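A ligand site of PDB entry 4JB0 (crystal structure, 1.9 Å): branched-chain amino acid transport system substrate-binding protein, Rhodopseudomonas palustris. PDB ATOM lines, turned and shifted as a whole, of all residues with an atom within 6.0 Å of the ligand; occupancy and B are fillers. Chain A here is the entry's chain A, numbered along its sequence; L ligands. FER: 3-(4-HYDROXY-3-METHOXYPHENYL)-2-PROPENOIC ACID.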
ATOM      1  N   LEU A  20      15.000 -11.463 -18.943  1.00  0.00           N
ATOM      2  CA  LEU A  20      16.358 -11.058 -19.289  1.00  0.00           C
ATOM      3  C   LEU A  20      17.363 -11.861 -18.492  1.00  0.00           C
ATOM      4  O   LEU A  20      18.330 -12.321 -19.051  1.00  0.00           O
ATOM      5  CB  LEU A  20      16.591  -9.554 -19.053  1.00  0.00           C
ATOM      6  CG  LEU A  20      16.058  -8.708 -20.246  1.00  0.00           C
ATOM      7  CD1 LEU A  20      14.559  -8.804 -20.449  1.00  0.00           C
ATOM      8  CD2 LEU A  20      16.403  -7.301 -20.041  1.00  0.00           C
ATOM      9  N   GLU A  24      20.577 -15.311 -19.264  1.00  0.00           N
ATOM     10  CA  GLU A  24      21.961 -15.091 -18.830  1.00  0.00           C
ATOM     11  C   GLU A  24      22.466 -16.217 -17.937  1.00  0.00           C
ATOM     12  O   GLU A  24      23.611 -16.689 -18.046  1.00  0.00           O
ATOM     13  CB  GLU A  24      22.092 -13.708 -18.124  1.00  0.00           C
ATOM     14  CG  GLU A  24      21.612 -12.596 -19.067  1.00  0.00           C
ATOM     15  CD  GLU A  24      21.776 -11.196 -18.579  1.00  0.00           C
ATOM     16  OE1 GLU A  24      21.562 -10.916 -17.375  1.00  0.00           O
ATOM     17  OE2 GLU A  24      22.119 -10.345 -19.431  1.00  0.00           O
ATOM     18  N   SER A  73      23.962  -6.525 -13.320  1.00  0.00           N
ATOM     19  CA  SER A  73      22.804  -7.388 -13.209  1.00  0.00           C
ATOM     20  C   SER A  73      22.157  -7.496 -14.604  1.00  0.00           C
ATOM     21  O   SER A  73      22.839  -7.374 -15.630  1.00  0.00           O
ATOM     22  CB  SER A  73      21.825  -6.797 -12.164  1.00  0.00           C
ATOM     23  OG  SER A  73      20.621  -7.555 -12.074  1.00  0.00           O
ATOM     24  N   SER A  74      20.870  -7.761 -14.627  1.00  0.00           N
ATOM     25  CA  SER A  74      20.143  -8.040 -15.871  1.00  0.00           C
ATOM     26  C   SER A  74      19.427  -6.782 -16.455  1.00  0.00           C
ATOM     27  O   SER A  74      19.100  -6.717 -17.675  1.00  0.00           O
ATOM     28  CB  SER A  74      19.123  -9.155 -15.558  1.00  0.00           C
ATOM     29  OG  SER A  74      19.825 -10.348 -15.184  1.00  0.00           O
ATOM     30  N   VAL A  75      19.166  -5.774 -15.600  1.00  0.00           N
ATOM     31  CA  VAL A  75      18.521  -4.526 -16.060  1.00  0.00           C
ATOM     32  C   VAL A  75      19.348  -3.330 -15.506  1.00  0.00           C
ATOM     33  O   VAL A  75      20.186  -3.536 -14.639  1.00  0.00           O
ATOM     34  CB  VAL A  75      17.008  -4.450 -15.677  1.00  0.00           C
ATOM     35  CG1 VAL A  75      16.182  -5.439 -16.588  1.00  0.00           C
ATOM     36  CG2 VAL A  75      16.808  -4.843 -14.219  1.00  0.00           C
ATOM     37  N   THR A  76      19.130  -2.125 -15.990  1.00  0.00           N
ATOM     38  CA  THR A  76      20.076  -1.049 -15.697  1.00  0.00           C
ATOM     39  C   THR A  76      20.115  -0.629 -14.194  1.00  0.00           C
ATOM     40  O   THR A  76      21.190  -0.470 -13.636  1.00  0.00           O
ATOM     41  CB  THR A  76      19.806   0.160 -16.615  1.00  0.00           C
ATOM     42  OG1 THR A  76      19.980  -0.231 -17.994  1.00  0.00           O
ATOM     43  CG2 THR A  76      20.831   1.346 -16.225  1.00  0.00           C
ATOM     44  N   PRO A  77      18.943  -0.438 -13.524  1.00  0.00           N
ATOM     45  CA  PRO A  77      19.100   0.058 -12.116  1.00  0.00           C
ATOM     46  C   PRO A  77      19.928  -0.841 -11.152  1.00  0.00           C
ATOM     47  O   PRO A  77      20.836  -0.314 -10.472  1.00  0.00           O
ATOM     48  CB  PRO A  77      17.645   0.290 -11.650  1.00  0.00           C
ATOM     49  CG  PRO A  77      16.863   0.527 -13.007  1.00  0.00           C
ATOM     50  CD  PRO A  77      17.535  -0.435 -13.971  1.00  0.00           C
ATOM     51  N   LEU A  96      26.084  -6.865 -17.079  1.00  0.00           N
ATOM     52  CA  LEU A  96      25.322  -7.715 -18.023  1.00  0.00           C
ATOM     53  C   LEU A  96      24.057  -7.012 -18.529  1.00  0.00           C
ATOM     54  O   LEU A  96      23.145  -7.644 -19.055  1.00  0.00           O
ATOM     55  CB  LEU A  96      24.994  -9.075 -17.381  1.00  0.00           C
ATOM     56  CG  LEU A  96      26.238  -9.872 -16.954  1.00  0.00           C
ATOM     57  CD1 LEU A  96      25.933 -11.209 -16.209  1.00  0.00           C
ATOM     58  CD2 LEU A  96      27.241 -10.125 -18.138  1.00  0.00           C
ATOM     59  N   ALA A  97      24.025  -5.683 -18.358  1.00  0.00           N
ATOM     60  CA  ALA A  97      22.951  -4.829 -18.770  1.00  0.00           C
ATOM     61  C   ALA A  97      23.656  -3.481 -19.004  1.00  0.00           C
ATOM     62  O   ALA A  97      24.738  -3.260 -18.481  1.00  0.00           O
ATOM     63  CB  ALA A  97      21.919  -4.702 -17.626  1.00  0.00           C
ATOM     64  N   PRO A  98      23.072  -2.589 -19.829  1.00  0.00           N
ATOM     65  CA  PRO A  98      23.659  -1.275 -20.100  1.00  0.00           C
ATOM     66  C   PRO A  98      23.701  -0.410 -18.833  1.00  0.00           C
ATOM     67  O   PRO A  98      22.933  -0.623 -17.878  1.00  0.00           O
ATOM     68  CB  PRO A  98      22.691  -0.632 -21.113  1.00  0.00           C
ATOM     69  CG  PRO A  98      21.696  -1.698 -21.448  1.00  0.00           C
ATOM     70  CD  PRO A  98      21.704  -2.697 -20.324  1.00  0.00           C
ATOM     71  N   PRO A 113      26.648  -5.357 -22.876  1.00  0.00           N
ATOM     72  CA  PRO A 113      25.676  -4.956 -23.891  1.00  0.00           C
ATOM     73  C   PRO A 113      26.167  -3.770 -24.717  1.00  0.00           C
ATOM     74  O   PRO A 113      27.008  -2.989 -24.251  1.00  0.00           O
ATOM     75  CB  PRO A 113      24.445  -4.526 -23.067  1.00  0.00           C
ATOM     76  CG  PRO A 113      24.569  -5.306 -21.770  1.00  0.00           C
ATOM     77  CD  PRO A 113      26.064  -5.302 -21.511  1.00  0.00           C
ATOM     78  N   GLN A 114      25.643  -3.637 -25.932  1.00  0.00           N
ATOM     79  CA  GLN A 114      26.021  -2.486 -26.772  1.00  0.00           C
ATOM     80  C   GLN A 114      25.692  -1.157 -26.102  1.00  0.00           C
ATOM     81  O   GLN A 114      24.606  -1.035 -25.475  1.00  0.00           O
ATOM     82  CB  GLN A 114      25.259  -2.564 -28.060  1.00  0.00           C
ATOM     83  CG  GLN A 114      25.716  -3.713 -28.957  1.00  0.00           C
ATOM     84  CD  GLN A 114      25.141  -5.083 -28.583  1.00  0.00           C
ATOM     85  OE1 GLN A 114      24.286  -5.225 -27.675  1.00  0.00           O
ATOM     86  NE2 GLN A 114      25.678  -6.127 -29.237  1.00  0.00           N
ATOM     87  N   TYR A 140      10.934   3.989 -19.985  1.00  0.00           N
ATOM     88  CA  TYR A 140      10.893   3.921 -18.548  1.00  0.00           C
ATOM     89  C   TYR A 140      11.267   5.252 -17.901  1.00  0.00           C
ATOM     90  O   TYR A 140      12.176   5.976 -18.378  1.00  0.00           O
ATOM     91  CB  TYR A 140      11.895   2.899 -18.028  1.00  0.00           C
ATOM     92  CG  TYR A 140      11.759   1.458 -18.471  1.00  0.00           C
ATOM     93  CD1 TYR A 140      10.515   0.859 -18.612  1.00  0.00           C
ATOM     94  CD2 TYR A 140      12.914   0.663 -18.605  1.00  0.00           C
ATOM     95  CE1 TYR A 140      10.401  -0.494 -18.961  1.00  0.00           C
ATOM     96  CE2 TYR A 140      12.815  -0.698 -18.939  1.00  0.00           C
ATOM     97  CZ  TYR A 140      11.531  -1.261 -19.106  1.00  0.00           C
ATOM     98  OH  TYR A 140      11.425  -2.596 -19.432  1.00  0.00           O
ATOM     99  N   ASP A 142      13.253   5.865 -15.647  1.00  0.00           N
ATOM    100  CA  ASP A 142      14.465   5.469 -14.910  1.00  0.00           C
ATOM    101  C   ASP A 142      15.725   5.665 -15.764  1.00  0.00           C
ATOM    102  O   ASP A 142      15.629   6.205 -16.870  1.00  0.00           O
ATOM    103  CB  ASP A 142      14.356   4.055 -14.252  1.00  0.00           C
ATOM    104  CG  ASP A 142      14.405   2.892 -15.231  1.00  0.00           C
ATOM    105  OD1 ASP A 142      13.823   1.822 -14.920  1.00  0.00           O
ATOM    106  OD2 ASP A 142      15.003   3.001 -16.309  1.00  0.00           O
ATOM    107  N   TYR A 144      17.625   3.689 -17.639  1.00  0.00           N
ATOM    108  CA  TYR A 144      17.643   3.143 -19.031  1.00  0.00           C
ATOM    109  C   TYR A 144      16.816   4.038 -19.942  1.00  0.00           C
ATOM    110  O   TYR A 144      17.252   4.348 -21.034  1.00  0.00           O
ATOM    111  CB  TYR A 144      17.040   1.736 -19.071  1.00  0.00           C
ATOM    112  CG  TYR A 144      17.128   1.028 -20.432  1.00  0.00           C
ATOM    113  CD1 TYR A 144      18.385   0.716 -21.005  1.00  0.00           C
ATOM    114  CD2 TYR A 144      15.963   0.692 -21.152  1.00  0.00           C
ATOM    115  CE1 TYR A 144      18.455   0.040 -22.256  1.00  0.00           C
ATOM    116  CE2 TYR A 144      16.022   0.042 -22.418  1.00  0.00           C
ATOM    117  CZ  TYR A 144      17.246  -0.290 -22.939  1.00  0.00           C
ATOM    118  OH  TYR A 144      17.281  -0.943 -24.130  1.00  0.00           O
ATOM    119  N   ARG A 171       8.414   0.623 -14.774  1.00  0.00           N
ATOM    120  CA  ARG A 171       8.582  -0.797 -15.104  1.00  0.00           C
ATOM    121  C   ARG A 171       7.424  -1.752 -14.823  1.00  0.00           C
ATOM    122  O   ARG A 171       7.097  -2.553 -15.693  1.00  0.00           O
ATOM    123  CB  ARG A 171       9.833  -1.363 -14.386  1.00  0.00           C
ATOM    124  CG  ARG A 171      11.052  -1.371 -15.244  1.00  0.00           C
ATOM    125  CD  ARG A 171      12.323  -1.627 -14.398  1.00  0.00           C
ATOM    126  NE  ARG A 171      13.463  -0.896 -14.998  1.00  0.00           N
ATOM    127  CZ  ARG A 171      14.220  -1.329 -16.005  1.00  0.00           C
ATOM    128  NH1 ARG A 171      14.035  -2.531 -16.541  1.00  0.00           N
ATOM    129  NH2 ARG A 171      15.217  -0.558 -16.456  1.00  0.00           N
ATOM    130  N   ALA A 195      12.371   0.578 -23.698  1.00  0.00           N
ATOM    131  CA  ALA A 195      11.913  -0.406 -22.696  1.00  0.00           C
ATOM    132  C   ALA A 195      12.608  -1.742 -23.024  1.00  0.00           C
ATOM    133  O   ALA A 195      13.531  -1.753 -23.842  1.00  0.00           O
ATOM    134  CB  ALA A 195      10.390  -0.524 -22.709  1.00  0.00           C
ATOM    135  N   SER A 196      12.193  -2.822 -22.364  1.00  0.00           N
ATOM    136  CA  SER A 196      12.931  -4.084 -22.414  1.00  0.00           C
ATOM    137  C   SER A 196      12.030  -5.258 -22.059  1.00  0.00           C
ATOM    138  O   SER A 196      10.981  -5.055 -21.415  1.00  0.00           O
ATOM    139  CB  SER A 196      14.171  -4.044 -21.465  1.00  0.00           C
ATOM    140  OG  SER A 196      13.741  -3.994 -20.098  1.00  0.00           O
ATOM    141  N   THR A 219      14.412  -0.941 -28.791  1.00  0.00           N
ATOM    142  CA  THR A 219      15.814  -1.106 -28.415  1.00  0.00           C
ATOM    143  C   THR A 219      16.241  -2.588 -28.314  1.00  0.00           C
ATOM    144  O   THR A 219      15.416  -3.532 -28.385  1.00  0.00           O
ATOM    145  CB  THR A 219      16.088  -0.402 -27.084  1.00  0.00           C
ATOM    146  OG1 THR A 219      15.538  -1.167 -26.005  1.00  0.00           O
ATOM    147  CG2 THR A 219      15.480   1.031 -27.062  1.00  0.00           C
ATOM    148  N   HIS A 220      17.507  -2.781 -28.052  1.00  0.00           N
ATOM    149  CA  HIS A 220      18.085  -4.088 -27.949  1.00  0.00           C
ATOM    150  C   HIS A 220      17.699  -4.744 -26.660  1.00  0.00           C
ATOM    151  O   HIS A 220      17.907  -5.927 -26.522  1.00  0.00           O
ATOM    152  CB  HIS A 220      19.610  -4.054 -28.197  1.00  0.00           C
ATOM    153  CG  HIS A 220      20.377  -3.130 -27.284  1.00  0.00           C
ATOM    154  ND1 HIS A 220      19.966  -1.843 -27.031  1.00  0.00           N
ATOM    155  CD2 HIS A 220      21.586  -3.272 -26.693  1.00  0.00           C
ATOM    156  CE1 HIS A 220      20.881  -1.232 -26.298  1.00  0.00           C
ATOM    157  NE2 HIS A 220      21.886  -2.068 -26.094  1.00  0.00           N
ATOM    158  N   GLY A 221      17.003  -3.998 -25.761  1.00  0.00           N
ATOM    159  CA  GLY A 221      16.428  -4.609 -24.567  1.00  0.00           C
ATOM    160  C   GLY A 221      15.237  -5.489 -24.881  1.00  0.00           C
ATOM    161  O   GLY A 221      14.780  -6.285 -24.030  1.00  0.00           O
ATOM    162  N   ALA A 222      14.722  -5.347 -26.094  1.00  0.00           N
ATOM    163  CA  ALA A 222      13.555  -6.114 -26.549  1.00  0.00           C
ATOM    164  C   ALA A 222      13.910  -7.428 -27.303  1.00  0.00           C
ATOM    165  O   ALA A 222      12.990  -8.233 -27.635  1.00  0.00           O
ATOM    166  CB  ALA A 222      12.691  -5.204 -27.445  1.00  0.00           C
ATOM    167  N   GLN A 279      19.409 -11.894 -27.250  1.00  0.00           N
ATOM    168  CA  GLN A 279      20.379 -10.829 -26.932  1.00  0.00           C
ATOM    169  C   GLN A 279      20.988 -11.116 -25.570  1.00  0.00           C
ATOM    170  O   GLN A 279      22.206 -10.893 -25.376  1.00  0.00           O
ATOM    171  CB  GLN A 279      19.642  -9.483 -26.983  1.00  0.00           C
ATOM    172  CG  GLN A 279      20.358  -8.314 -26.398  1.00  0.00           C
ATOM    173  CD  GLN A 279      21.334  -7.741 -27.392  1.00  0.00           C
ATOM    174  OE1 GLN A 279      21.365  -8.183 -28.505  1.00  0.00           O
ATOM    175  NE2 GLN A 279      22.026  -6.665 -27.038  1.00  0.00           N
ATOM    176  N   PHE A 280      20.160 -11.642 -24.635  1.00  0.00           N
ATOM    177  CA  PHE A 280      20.580 -11.601 -23.229  1.00  0.00           C
ATOM    178  C   PHE A 280      21.501 -12.772 -22.855  1.00  0.00           C
ATOM    179  O   PHE A 280      22.500 -12.586 -22.213  1.00  0.00           O
ATOM    180  CB  PHE A 280      19.348 -11.529 -22.324  1.00  0.00           C
ATOM    181  CG  PHE A 280      18.284 -10.648 -22.886  1.00  0.00           C
ATOM    182  CD1 PHE A 280      18.575  -9.338 -23.248  1.00  0.00           C
ATOM    183  CD2 PHE A 280      17.026 -11.137 -23.129  1.00  0.00           C
ATOM    184  CE1 PHE A 280      17.591  -8.515 -23.783  1.00  0.00           C
ATOM    185  CE2 PHE A 280      16.020 -10.327 -23.647  1.00  0.00           C
ATOM    186  CZ  PHE A 280      16.323  -9.031 -24.003  1.00  0.00           C
ATOM    187  N   HIS A 283      25.300 -12.152 -23.328  1.00  0.00           N
ATOM    188  CA  HIS A 283      26.148 -11.290 -22.461  1.00  0.00           C
ATOM    189  C   HIS A 283      26.947 -12.074 -21.468  1.00  0.00           C
ATOM    190  O   HIS A 283      28.111 -11.792 -21.286  1.00  0.00           O
ATOM    191  CB  HIS A 283      25.328 -10.223 -21.766  1.00  0.00           C
ATOM    192  CG  HIS A 283      24.594  -9.310 -22.722  1.00  0.00           C
ATOM    193  ND1 HIS A 283      25.136  -8.880 -23.913  1.00  0.00           N
ATOM    194  CD2 HIS A 283      23.363  -8.742 -22.641  1.00  0.00           C
ATOM    195  CE1 HIS A 283      24.271  -8.106 -24.543  1.00  0.00           C
ATOM    196  NE2 HIS A 283      23.183  -8.020 -23.799  1.00  0.00           N
ATOM    197  N   GLN A 327      28.621 -11.092 -29.517  1.00  0.00           N
ATOM    198  CA  GLN A 327      27.937  -9.811 -29.693  1.00  0.00           C
ATOM    199  C   GLN A 327      28.794  -8.705 -30.342  1.00  0.00           C
ATOM    200  O   GLN A 327      28.283  -7.652 -30.653  1.00  0.00           O
ATOM    201  CB  GLN A 327      27.461  -9.277 -28.341  1.00  0.00           C
ATOM    202  CG  GLN A 327      26.250 -10.073 -27.811  1.00  0.00           C
ATOM    203  CD  GLN A 327      24.937  -9.815 -28.567  1.00  0.00           C
ATOM    204  OE1 GLN A 327      24.904  -9.804 -29.796  1.00  0.00           O
ATOM    205  NE2 GLN A 327      23.836  -9.655 -27.822  1.00  0.00           N
HETATM  206  C4  FER L   1      20.518  -5.537 -23.241  1.00  0.00           C
HETATM  207  C5  FER L   1      19.978  -4.287 -23.520  1.00  0.00           C
HETATM  208  C6  FER L   1      19.071  -3.754 -22.624  1.00  0.00           C
HETATM  209  C3  FER L   1      20.165  -6.230 -22.102  1.00  0.00           C
HETATM  210  C2  FER L   1      19.249  -5.683 -21.188  1.00  0.00           C
HETATM  211  C1  FER L   1      18.709  -4.433 -21.467  1.00  0.00           C
HETATM  212  C10 FER L   1      20.296  -8.188 -20.641  1.00  0.00           C
HETATM  213  C7  FER L   1      17.750  -3.930 -20.442  1.00  0.00           C
HETATM  214  C8  FER L   1      17.758  -2.685 -19.967  1.00  0.00           C
HETATM  215  C9  FER L   1      16.826  -2.310 -18.871  1.00  0.00           C
HETATM  216  O1  FER L   1      15.645  -2.755 -18.812  1.00  0.00           O
HETATM  217  O2  FER L   1      17.317  -1.608 -17.945  1.00  0.00           O
HETATM  218  O4  FER L   1      21.411  -6.076 -24.088  1.00  0.00           O
HETATM  219  O3  FER L   1      20.706  -7.469 -21.831  1.00  0.00           O
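Leu 20 touches the ligand. OE2 of Glu 24 touches C10 of the ligand, 3.1 Å away. O of Ser 74 touches C10 of the ligand, 3.5 Å away. CG1 of Val 75 touches O1 of the ligand (3.5 Å). Leu 96 touches the ligand. Pro 98 touches the ligand (CG to C6, 3.5 Å). CB of Pro 113 touches O4 of the ligand, at 3.6 Å. Tyr 140 touches the ligand. Tyr 144 touches the ligand (CB to O2, 3.5 Å). His 220 touches the ligand (CD2 to C5, 3.7 Å). CA of Gly 221 touches C6 of the ligand, 3.4 Å away. Phe 280 touches the ligand (CD1 to O3, 3.2 Å). Hydrophobic or aromatic side chains within 4 Å of the ligand: Leu 20, Val 75, Pro 98, Pro 113, Tyr 140, Tyr 144, His 220, Phe 280 and His 283. 17 residues have an atom within 4 Å of the ligand: Leu 20, Glu 24, Ser 74, Val 75, Thr 76, Leu 96, Pro 98, Pro 113, Tyr 140, Tyr 144, Arg 171, Ser 196, His 220, Gly 221, Gln 279, Phe 280 and His 283.
An oxygen (O4) of the ligand lies within hydrogen-bond range of the side-chain amide nitrogen (NE2) of Gln 279, at 3.1 Å. An oxygen (O1) of the ligand is in hydrogen-bond range of the side-chain hydroxyl (OG) of Ser 196 (2.6 Å). O2 of the ligand is in salt-bridge range of NH2 of Arg 171 (2.8 Å). O4 of the ligand is in hydrogen-bond range of NE2 of His 283, at 2.6 Å. O2 of the ligand sits at hydrogen-bond distance from OG1 of Thr 76 (3.0 Å). N of Thr 76 is in hydrogen-bond range of O2 of the ligand.
NE2 of His 220 lies within hydrogen-bond range of O of Gln 114. OG of Ser 74 is in hydrogen-bond range of OE1 of Glu 24, 2.9 Å away. A ring nitrogen (NE2) of His 283 sits at hydrogen-bond distance from the backbone carbonyl oxygen of Gln 279 (3.4 Å). The backbone NH of Tyr 144 sits at hydrogen-bond distance from the side-chain carboxylate of Asp 142, at 3.0 Å. OG of Ser 196 is in hydrogen-bond range of OH of Tyr 140, 2.8 Å away. The side-chain hydroxyl of Thr 76 lies within hydrogen-bond range of the backbone carbonyl oxygen of Pro 98 (3.0 Å). The side-chain hydroxyl of Tyr 144 sits at hydrogen-bond distance from the side-chain hydroxyl of Thr 219. OG1 of Thr 219 sits close to N of Gly 221.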
